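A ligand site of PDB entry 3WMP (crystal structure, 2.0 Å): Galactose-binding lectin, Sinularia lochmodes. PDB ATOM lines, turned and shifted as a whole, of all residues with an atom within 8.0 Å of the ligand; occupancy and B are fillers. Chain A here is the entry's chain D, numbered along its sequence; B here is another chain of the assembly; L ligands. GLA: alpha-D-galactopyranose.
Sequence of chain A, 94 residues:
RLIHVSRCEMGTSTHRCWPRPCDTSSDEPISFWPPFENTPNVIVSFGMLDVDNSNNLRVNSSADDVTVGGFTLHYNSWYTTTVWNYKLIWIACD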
ATOM      1  N   ASN A  55      13.752 -11.315 -21.778  1.00  0.00           N
ATOM      2  CA  ASN A  55      14.916 -12.030 -21.273  1.00  0.00           C
ATOM      3  C   ASN A  55      14.690 -12.364 -19.792  1.00  0.00           C
ATOM      4  O   ASN A  55      13.698 -11.921 -19.217  1.00  0.00           O
ATOM      5  CB  ASN A  55      16.196 -11.222 -21.469  1.00  0.00           C
ATOM      6  CG  ASN A  55      16.527 -11.047 -22.948  1.00  0.00           C
ATOM      7  OD1 ASN A  55      17.097 -11.931 -23.574  1.00  0.00           O
ATOM      8  ND2 ASN A  55      16.156  -9.894 -23.497  1.00  0.00           N
ATOM      9  N   ASN A  56      15.576 -13.144 -19.208  1.00  0.00           N
ATOM     10  CA  ASN A  56      15.429 -13.533 -17.814  1.00  0.00           C
ATOM     11  C   ASN A  56      15.478 -12.345 -16.868  1.00  0.00           C
ATOM     12  O   ASN A  56      16.068 -11.309 -17.179  1.00  0.00           O
ATOM     13  CB  ASN A  56      16.510 -14.540 -17.413  1.00  0.00           C
ATOM     14  CG  ASN A  56      16.284 -15.905 -18.019  1.00  0.00           C
ATOM     15  OD1 ASN A  56      15.217 -16.166 -18.574  1.00  0.00           O
ATOM     16  ND2 ASN A  56      17.265 -16.790 -17.906  1.00  0.00           N
ATOM     17  N   LEU A  57      14.833 -12.496 -15.718  1.00  0.00           N
ATOM     18  CA  LEU A  57      14.884 -11.466 -14.707  1.00  0.00           C
ATOM     19  C   LEU A  57      16.139 -11.671 -13.869  1.00  0.00           C
ATOM     20  O   LEU A  57      16.267 -12.666 -13.174  1.00  0.00           O
ATOM     21  CB  LEU A  57      13.644 -11.531 -13.799  1.00  0.00           C
ATOM     22  CG  LEU A  57      13.564 -10.472 -12.678  1.00  0.00           C
ATOM     23  CD1 LEU A  57      12.109 -10.056 -12.471  1.00  0.00           C
ATOM     24  CD2 LEU A  57      14.157 -11.005 -11.387  1.00  0.00           C
ATOM     25  N   ARG A  58      17.072 -10.736 -13.976  1.00  0.00           N
ATOM     26  CA  ARG A  58      18.294 -10.799 -13.178  1.00  0.00           C
ATOM     27  C   ARG A  58      18.540  -9.460 -12.463  1.00  0.00           C
ATOM     28  O   ARG A  58      18.972  -8.479 -13.090  1.00  0.00           O
ATOM     29  CB  ARG A  58      19.516 -11.133 -14.048  1.00  0.00           C
ATOM     30  CG  ARG A  58      19.391 -12.414 -14.869  1.00  0.00           C
ATOM     31  CD  ARG A  58      20.588 -12.571 -15.808  1.00  0.00           C
ATOM     32  NE  ARG A  58      20.453 -13.726 -16.711  1.00  0.00           N
ATOM     33  CZ  ARG A  58      19.990 -13.665 -17.953  1.00  0.00           C
ATOM     34  NH1 ARG A  58      19.609 -12.500 -18.473  1.00  0.00           N
ATOM     35  NH2 ARG A  58      19.892 -14.774 -18.682  1.00  0.00           N
ATOM     36  N   TRP A  78      22.589  -8.172 -14.873  1.00  0.00           N
ATOM     37  CA  TRP A  78      23.694  -8.753 -15.637  1.00  0.00           C
ATOM     38  C   TRP A  78      23.208  -9.482 -16.887  1.00  0.00           C
ATOM     39  O   TRP A  78      21.996  -9.705 -17.054  1.00  0.00           O
ATOM     40  CB  TRP A  78      24.578  -9.653 -14.771  1.00  0.00           C
ATOM     41  CG  TRP A  78      23.949 -10.904 -14.238  1.00  0.00           C
ATOM     42  CD1 TRP A  78      24.038 -12.161 -14.758  1.00  0.00           C
ATOM     43  CD2 TRP A  78      23.130 -11.019 -13.052  1.00  0.00           C
ATOM     44  NE1 TRP A  78      23.337 -13.049 -13.983  1.00  0.00           N
ATOM     45  CE2 TRP A  78      22.766 -12.375 -12.929  1.00  0.00           C
ATOM     46  CE3 TRP A  78      22.677 -10.111 -12.097  1.00  0.00           C
ATOM     47  CZ2 TRP A  78      21.974 -12.848 -11.879  1.00  0.00           C
ATOM     48  CZ3 TRP A  78      21.884 -10.572 -11.052  1.00  0.00           C
ATOM     49  CH2 TRP A  78      21.536 -11.934 -10.964  1.00  0.00           C
ATOM     50  N   TYR A  79      24.143  -9.832 -17.756  1.00  0.00           N
ATOM     51  CA  TYR A  79      23.858 -10.522 -19.003  1.00  0.00           C
ATOM     52  C   TYR A  79      22.848  -9.779 -19.874  1.00  0.00           C
ATOM     53  O   TYR A  79      22.996  -8.574 -20.099  1.00  0.00           O
ATOM     54  CB  TYR A  79      23.399 -11.959 -18.747  1.00  0.00           C
ATOM     55  CG  TYR A  79      23.641 -12.894 -19.910  1.00  0.00           C
ATOM     56  CD1 TYR A  79      24.903 -13.003 -20.491  1.00  0.00           C
ATOM     57  CD2 TYR A  79      22.608 -13.671 -20.436  1.00  0.00           C
ATOM     58  CE1 TYR A  79      25.123 -13.860 -21.565  1.00  0.00           C
ATOM     59  CE2 TYR A  79      22.828 -14.527 -21.510  1.00  0.00           C
ATOM     60  CZ  TYR A  79      24.087 -14.618 -22.065  1.00  0.00           C
ATOM     61  OH  TYR A  79      24.310 -15.466 -23.121  1.00  0.00           O
ATOM     62  N   THR A  80      21.805 -10.468 -20.327  1.00  0.00           N
ATOM     63  CA  THR A  80      20.843  -9.895 -21.270  1.00  0.00           C
ATOM     64  C   THR A  80      19.621  -9.262 -20.669  1.00  0.00           C
ATOM     65  O   THR A  80      18.686  -8.903 -21.389  1.00  0.00           O
ATOM     66  CB  THR A  80      20.364 -10.984 -22.269  1.00  0.00           C
ATOM     67  OG1 THR A  80      19.856 -12.112 -21.535  1.00  0.00           O
ATOM     68  CG2 THR A  80      21.495 -11.444 -23.185  1.00  0.00           C
ATOM     69  N   THR A  81      19.595  -9.117 -19.352  1.00  0.00           N
ATOM     70  CA  THR A  81      18.436  -8.552 -18.694  1.00  0.00           C
ATOM     71  C   THR A  81      18.184  -7.083 -18.978  1.00  0.00           C
ATOM     72  O   THR A  81      19.123  -6.287 -19.030  1.00  0.00           O
ATOM     73  CB  THR A  81      18.534  -8.758 -17.151  1.00  0.00           C
ATOM     74  OG1 THR A  81      18.398 -10.157 -16.856  1.00  0.00           O
ATOM     75  CG2 THR A  81      17.437  -7.987 -16.435  1.00  0.00           C
ATOM     76  N   ARG B  16      23.546 -19.629  -4.985  1.00  0.00           N
ATOM     77  CA  ARG B  16      23.990 -19.632  -6.386  1.00  0.00           C
ATOM     78  C   ARG B  16      23.826 -21.082  -6.871  1.00  0.00           C
ATOM     79  O   ARG B  16      24.470 -22.005  -6.368  1.00  0.00           O
ATOM     80  CB  ARG B  16      25.436 -19.148  -6.510  1.00  0.00           C
ATOM     81  CG  ARG B  16      25.604 -17.670  -6.118  1.00  0.00           C
ATOM     82  CD  ARG B  16      26.898 -17.083  -6.658  1.00  0.00           C
ATOM     83  NE  ARG B  16      26.672 -15.826  -7.373  1.00  0.00           N
ATOM     84  CZ  ARG B  16      26.236 -15.752  -8.626  1.00  0.00           C
ATOM     85  NH1 ARG B  16      25.979 -16.854  -9.319  1.00  0.00           N
ATOM     86  NH2 ARG B  16      26.053 -14.566  -9.201  1.00  0.00           N
ATOM     87  N   TRP B  18      22.924 -21.873 -10.638  1.00  0.00           N
ATOM     88  CA  TRP B  18      23.299 -21.998 -12.047  1.00  0.00           C
ATOM     89  C   TRP B  18      24.649 -22.681 -12.164  1.00  0.00           C
ATOM     90  O   TRP B  18      25.572 -22.366 -11.407  1.00  0.00           O
ATOM     91  CB  TRP B  18      23.356 -20.596 -12.689  1.00  0.00           C
ATOM     92  CG  TRP B  18      23.918 -20.579 -14.076  1.00  0.00           C
ATOM     93  CD1 TRP B  18      25.228 -20.376 -14.433  1.00  0.00           C
ATOM     94  CD2 TRP B  18      23.206 -20.760 -15.304  1.00  0.00           C
ATOM     95  NE1 TRP B  18      25.362 -20.418 -15.808  1.00  0.00           N
ATOM     96  CE2 TRP B  18      24.130 -20.656 -16.357  1.00  0.00           C
ATOM     97  CE3 TRP B  18      21.854 -21.000 -15.607  1.00  0.00           C
ATOM     98  CZ2 TRP B  18      23.754 -20.789 -17.700  1.00  0.00           C
ATOM     99  CZ3 TRP B  18      21.489 -21.130 -16.931  1.00  0.00           C
ATOM    100  CH2 TRP B  18      22.437 -21.024 -17.967  1.00  0.00           C
ATOM    101  N   PRO B  19      24.832 -23.566 -13.172  1.00  0.00           N
ATOM    102  CA  PRO B  19      23.918 -23.985 -14.240  1.00  0.00           C
ATOM    103  C   PRO B  19      22.779 -24.904 -13.846  1.00  0.00           C
ATOM    104  O   PRO B  19      22.050 -25.378 -14.706  1.00  0.00           O
ATOM    105  CB  PRO B  19      24.841 -24.632 -15.255  1.00  0.00           C
ATOM    106  CG  PRO B  19      25.836 -25.312 -14.379  1.00  0.00           C
ATOM    107  CD  PRO B  19      26.054 -24.396 -13.184  1.00  0.00           C
ATOM    108  N   ARG B  20      22.665 -25.186 -12.567  1.00  0.00           N
ATOM    109  CA  ARG B  20      21.555 -26.009 -12.124  1.00  0.00           C
ATOM    110  C   ARG B  20      20.433 -25.110 -11.600  1.00  0.00           C
ATOM    111  O   ARG B  20      20.663 -23.944 -11.271  1.00  0.00           O
ATOM    112  CB  ARG B  20      21.986 -26.875 -10.903  1.00  0.00           C
ATOM    113  CG  ARG B  20      23.277 -27.675 -11.121  1.00  0.00           C
ATOM    114  CD  ARG B  20      23.744 -28.331  -9.829  1.00  0.00           C
ATOM    115  NE  ARG B  20      24.915 -29.207 -10.012  1.00  0.00           N
ATOM    116  CZ  ARG B  20      26.163 -28.781 -10.163  1.00  0.00           C
ATOM    117  NH1 ARG B  20      26.443 -27.481 -10.165  1.00  0.00           N
ATOM    118  NH2 ARG B  20      27.145 -29.656 -10.314  1.00  0.00           N
ATOM    119  N   LEU B  49      17.888 -11.868  -7.354  1.00  0.00           N
ATOM    120  CA  LEU B  49      16.992 -12.826  -7.984  1.00  0.00           C
ATOM    121  C   LEU B  49      17.329 -13.063  -9.457  1.00  0.00           C
ATOM    122  O   LEU B  49      17.648 -12.121 -10.192  1.00  0.00           O
ATOM    123  CB  LEU B  49      15.539 -12.342  -7.833  1.00  0.00           C
ATOM    124  CG  LEU B  49      14.409 -13.359  -8.024  1.00  0.00           C
ATOM    125  CD1 LEU B  49      14.634 -14.590  -7.153  1.00  0.00           C
ATOM    126  CD2 LEU B  49      13.064 -12.707  -7.691  1.00  0.00           C
ATOM    127  N   ASP B  50      17.270 -14.318  -9.885  1.00  0.00           N
ATOM    128  CA  ASP B  50      17.586 -14.700 -11.261  1.00  0.00           C
ATOM    129  C   ASP B  50      16.565 -15.765 -11.650  1.00  0.00           C
ATOM    130  O   ASP B  50      16.687 -16.937 -11.284  1.00  0.00           O
ATOM    131  CB  ASP B  50      19.025 -15.239 -11.305  1.00  0.00           C
ATOM    132  CG  ASP B  50      19.439 -15.699 -12.705  1.00  0.00           C
ATOM    133  OD1 ASP B  50      20.596 -16.147 -12.857  1.00  0.00           O
ATOM    134  OD2 ASP B  50      18.627 -15.605 -13.656  1.00  0.00           O
ATOM    135  N   VAL B  51      15.562 -15.340 -12.413  1.00  0.00           N
ATOM    136  CA  VAL B  51      14.443 -16.224 -12.759  1.00  0.00           C
ATOM    137  C   VAL B  51      14.243 -16.373 -14.249  1.00  0.00           C
ATOM    138  O   VAL B  51      14.286 -15.387 -14.991  1.00  0.00           O
ATOM    139  CB  VAL B  51      13.131 -15.640 -12.107  1.00  0.00           C
ATOM    140  CG1 VAL B  51      11.941 -16.530 -12.450  1.00  0.00           C
ATOM    141  CG2 VAL B  51      13.294 -15.530 -10.592  1.00  0.00           C
ATOM    142  N   ASP B  52      14.020 -17.594 -14.699  1.00  0.00           N
ATOM    143  CA  ASP B  52      13.848 -17.853 -16.129  1.00  0.00           C
ATOM    144  C   ASP B  52      12.496 -17.389 -16.637  1.00  0.00           C
ATOM    145  O   ASP B  52      11.452 -17.662 -16.022  1.00  0.00           O
ATOM    146  CB  ASP B  52      14.050 -19.349 -16.430  1.00  0.00           C
ATOM    147  CG  ASP B  52      14.527 -19.590 -17.846  1.00  0.00           C
ATOM    148  OD1 ASP B  52      13.704 -19.488 -18.776  1.00  0.00           O
ATOM    149  OD2 ASP B  52      15.744 -19.861 -18.037  1.00  0.00           O
ATOM    150  N   ASN B  53      12.502 -16.703 -17.779  1.00  0.00           N
ATOM    151  CA  ASN B  53      11.295 -16.164 -18.382  1.00  0.00           C
ATOM    152  C   ASN B  53      10.446 -17.192 -19.121  1.00  0.00           C
ATOM    153  O   ASN B  53       9.350 -16.882 -19.588  1.00  0.00           O
ATOM    154  CB  ASN B  53      11.660 -15.035 -19.350  1.00  0.00           C
ATOM    155  CG  ASN B  53      12.411 -15.529 -20.567  1.00  0.00           C
ATOM    156  OD1 ASN B  53      12.902 -16.668 -20.574  1.00  0.00           O
ATOM    157  ND2 ASN B  53      12.513 -14.694 -21.595  1.00  0.00           N
ATOM    158  N   THR B  82      11.320 -21.681 -12.810  1.00  0.00           N
ATOM    159  CA  THR B  82      12.722 -22.060 -12.756  1.00  0.00           C
ATOM    160  C   THR B  82      13.573 -20.908 -12.223  1.00  0.00           C
ATOM    161  O   THR B  82      13.672 -19.856 -12.850  1.00  0.00           O
ATOM    162  CB  THR B  82      13.252 -22.453 -14.141  1.00  0.00           C
ATOM    163  OG1 THR B  82      12.558 -23.617 -14.605  1.00  0.00           O
ATOM    164  CG2 THR B  82      14.741 -22.753 -14.073  1.00  0.00           C
ATOM    165  N   VAL B  83      14.179 -21.117 -11.046  1.00  0.00           N
ATOM    166  CA  VAL B  83      15.017 -20.100 -10.412  1.00  0.00           C
ATOM    167  C   VAL B  83      16.482 -20.516 -10.486  1.00  0.00           C
ATOM    168  O   VAL B  83      16.844 -21.628 -10.101  1.00  0.00           O
ATOM    169  CB  VAL B  83      14.607 -19.891  -8.947  1.00  0.00           C
ATOM    170  CG1 VAL B  83      15.490 -18.848  -8.300  1.00  0.00           C
ATOM    171  CG2 VAL B  83      13.148 -19.452  -8.874  1.00  0.00           C
ATOM    172  N   TRP B  84      17.331 -19.609 -10.970  1.00  0.00           N
ATOM    173  CA  TRP B  84      18.755 -19.885 -11.172  1.00  0.00           C
ATOM    174  C   TRP B  84      19.653 -19.450 -10.031  1.00  0.00           C
ATOM    175  O   TRP B  84      20.661 -20.109  -9.740  1.00  0.00           O
ATOM    176  CB  TRP B  84      19.240 -19.207 -12.448  1.00  0.00           C
ATOM    177  CG  TRP B  84      18.584 -19.725 -13.692  1.00  0.00           C
ATOM    178  CD1 TRP B  84      17.785 -19.025 -14.556  1.00  0.00           C
ATOM    179  CD2 TRP B  84      18.668 -21.053 -14.212  1.00  0.00           C
ATOM    180  NE1 TRP B  84      17.379 -19.840 -15.587  1.00  0.00           N
ATOM    181  CE2 TRP B  84      17.902 -21.094 -15.397  1.00  0.00           C
ATOM    182  CE3 TRP B  84      19.318 -22.219 -13.794  1.00  0.00           C
ATOM    183  CZ2 TRP B  84      17.769 -22.243 -16.168  1.00  0.00           C
ATOM    184  CZ3 TRP B  84      19.193 -23.374 -14.563  1.00  0.00           C
ATOM    185  CH2 TRP B  84      18.421 -23.370 -15.735  1.00  0.00           C
ATOM    186  N   ASN B  85      19.297 -18.336  -9.417  1.00  0.00           N
ATOM    187  CA  ASN B  85      20.035 -17.767  -8.303  1.00  0.00           C
ATOM    188  C   ASN B  85      19.108 -16.883  -7.468  1.00  0.00           C
ATOM    189  O   ASN B  85      18.164 -16.292  -8.007  1.00  0.00           O
ATOM    190  CB  ASN B  85      21.171 -16.837  -8.824  1.00  0.00           C
ATOM    191  CG  ASN B  85      22.249 -17.584  -9.604  1.00  0.00           C
ATOM    192  OD1 ASN B  85      23.065 -18.309  -9.035  1.00  0.00           O
ATOM    193  ND2 ASN B  85      22.243 -17.413 -10.922  1.00  0.00           N
HETATM  194  C1  GLA L   1      23.135 -16.427 -18.093  1.00  0.00           C
HETATM  195  C2  GLA L   1      23.973 -15.812 -16.973  1.00  0.00           C
HETATM  196  C3  GLA L   1      23.967 -16.752 -15.754  1.00  0.00           C
HETATM  197  C4  GLA L   1      22.526 -16.989 -15.335  1.00  0.00           C
HETATM  198  C5  GLA L   1      21.756 -17.599 -16.514  1.00  0.00           C
HETATM  199  C6  GLA L   1      20.291 -17.843 -16.188  1.00  0.00           C
HETATM  200  O1  GLA L   1      23.701 -17.616 -18.516  1.00  0.00           O
HETATM  201  O2  GLA L   1      25.303 -15.606 -17.414  1.00  0.00           O
HETATM  202  O3  GLA L   1      24.689 -16.168 -14.688  1.00  0.00           O
HETATM  203  O4  GLA L   1      21.934 -15.749 -14.966  1.00  0.00           O
HETATM  204  O5  GLA L   1      21.794 -16.693 -17.644  1.00  0.00           O
HETATM  205  O6  GLA L   1      19.593 -16.617 -16.042  1.00  0.00           O
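ND2 of Asn 85 of chain B lies within hydrogen-bond range of OD1 of Asp 50 of chain B. The guanidinium group of Arg 58 sits at hydrogen-bond distance from the side-chain hydroxyl of Thr 80. The backbone carbonyl oxygen (O) of Asn 56 sits at hydrogen-bond distance from the side-chain hydroxyl (OG1) of Thr 81 (2.6 Å). OG1 of Thr 81 lies within hydrogen-bond range of NH1 of Arg 58, at 3.1 Å. O of Trp 84 of chain B sits at hydrogen-bond distance from N of Trp 18 of chain B (3.0 Å). The side-chain carboxylate of Asp 52 of chain B sits at hydrogen-bond distance from the side-chain amide nitrogen of Asn 56, at 3.4 Å. O of Asp 50 of chain B is in hydrogen-bond range of N of Trp 84 of chain B (2.8 Å). OD2 of Asp 52 of chain B lies within hydrogen-bond range of NE1 of Trp 84 of chain B (2.9 Å).
Residues that only touch the ligand: Tyr 79 (3.7 Å), Trp 18 of chain B (3.3 Å) and Trp 84 of chain B (3.2 Å). Hydrophobic or aromatic side chains that line the ligand: Tyr 79, Trp 18 of chain B and Trp 84 of chain B. Seven residues have an atom within 4 Å of the ligand: Asn 56, Arg 58, Trp 78, Tyr 79, Trp 18 of chain B, Asp 50 of chain B and Trp 84 of chain B. The nearest printed residue that does not touch the ligand is Asn 85 of chain B (4.4 Å).
OD1 of Asp 50 of chain B lies within hydrogen-bond range of O4 of the ligand (2.5 Å). ND2 of Asn 56 is in hydrogen-bond range of O6 of the ligand (3.0 Å). The guanidinium group (NH2) of Arg 58 sits at hydrogen-bond distance from an oxygen (O5) of the ligand (2.9 Å). The indole nitrogen (NE1) of Trp 78 lies within hydrogen-bond range of an oxygen (O4) of the ligand, 3.2 Å away.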
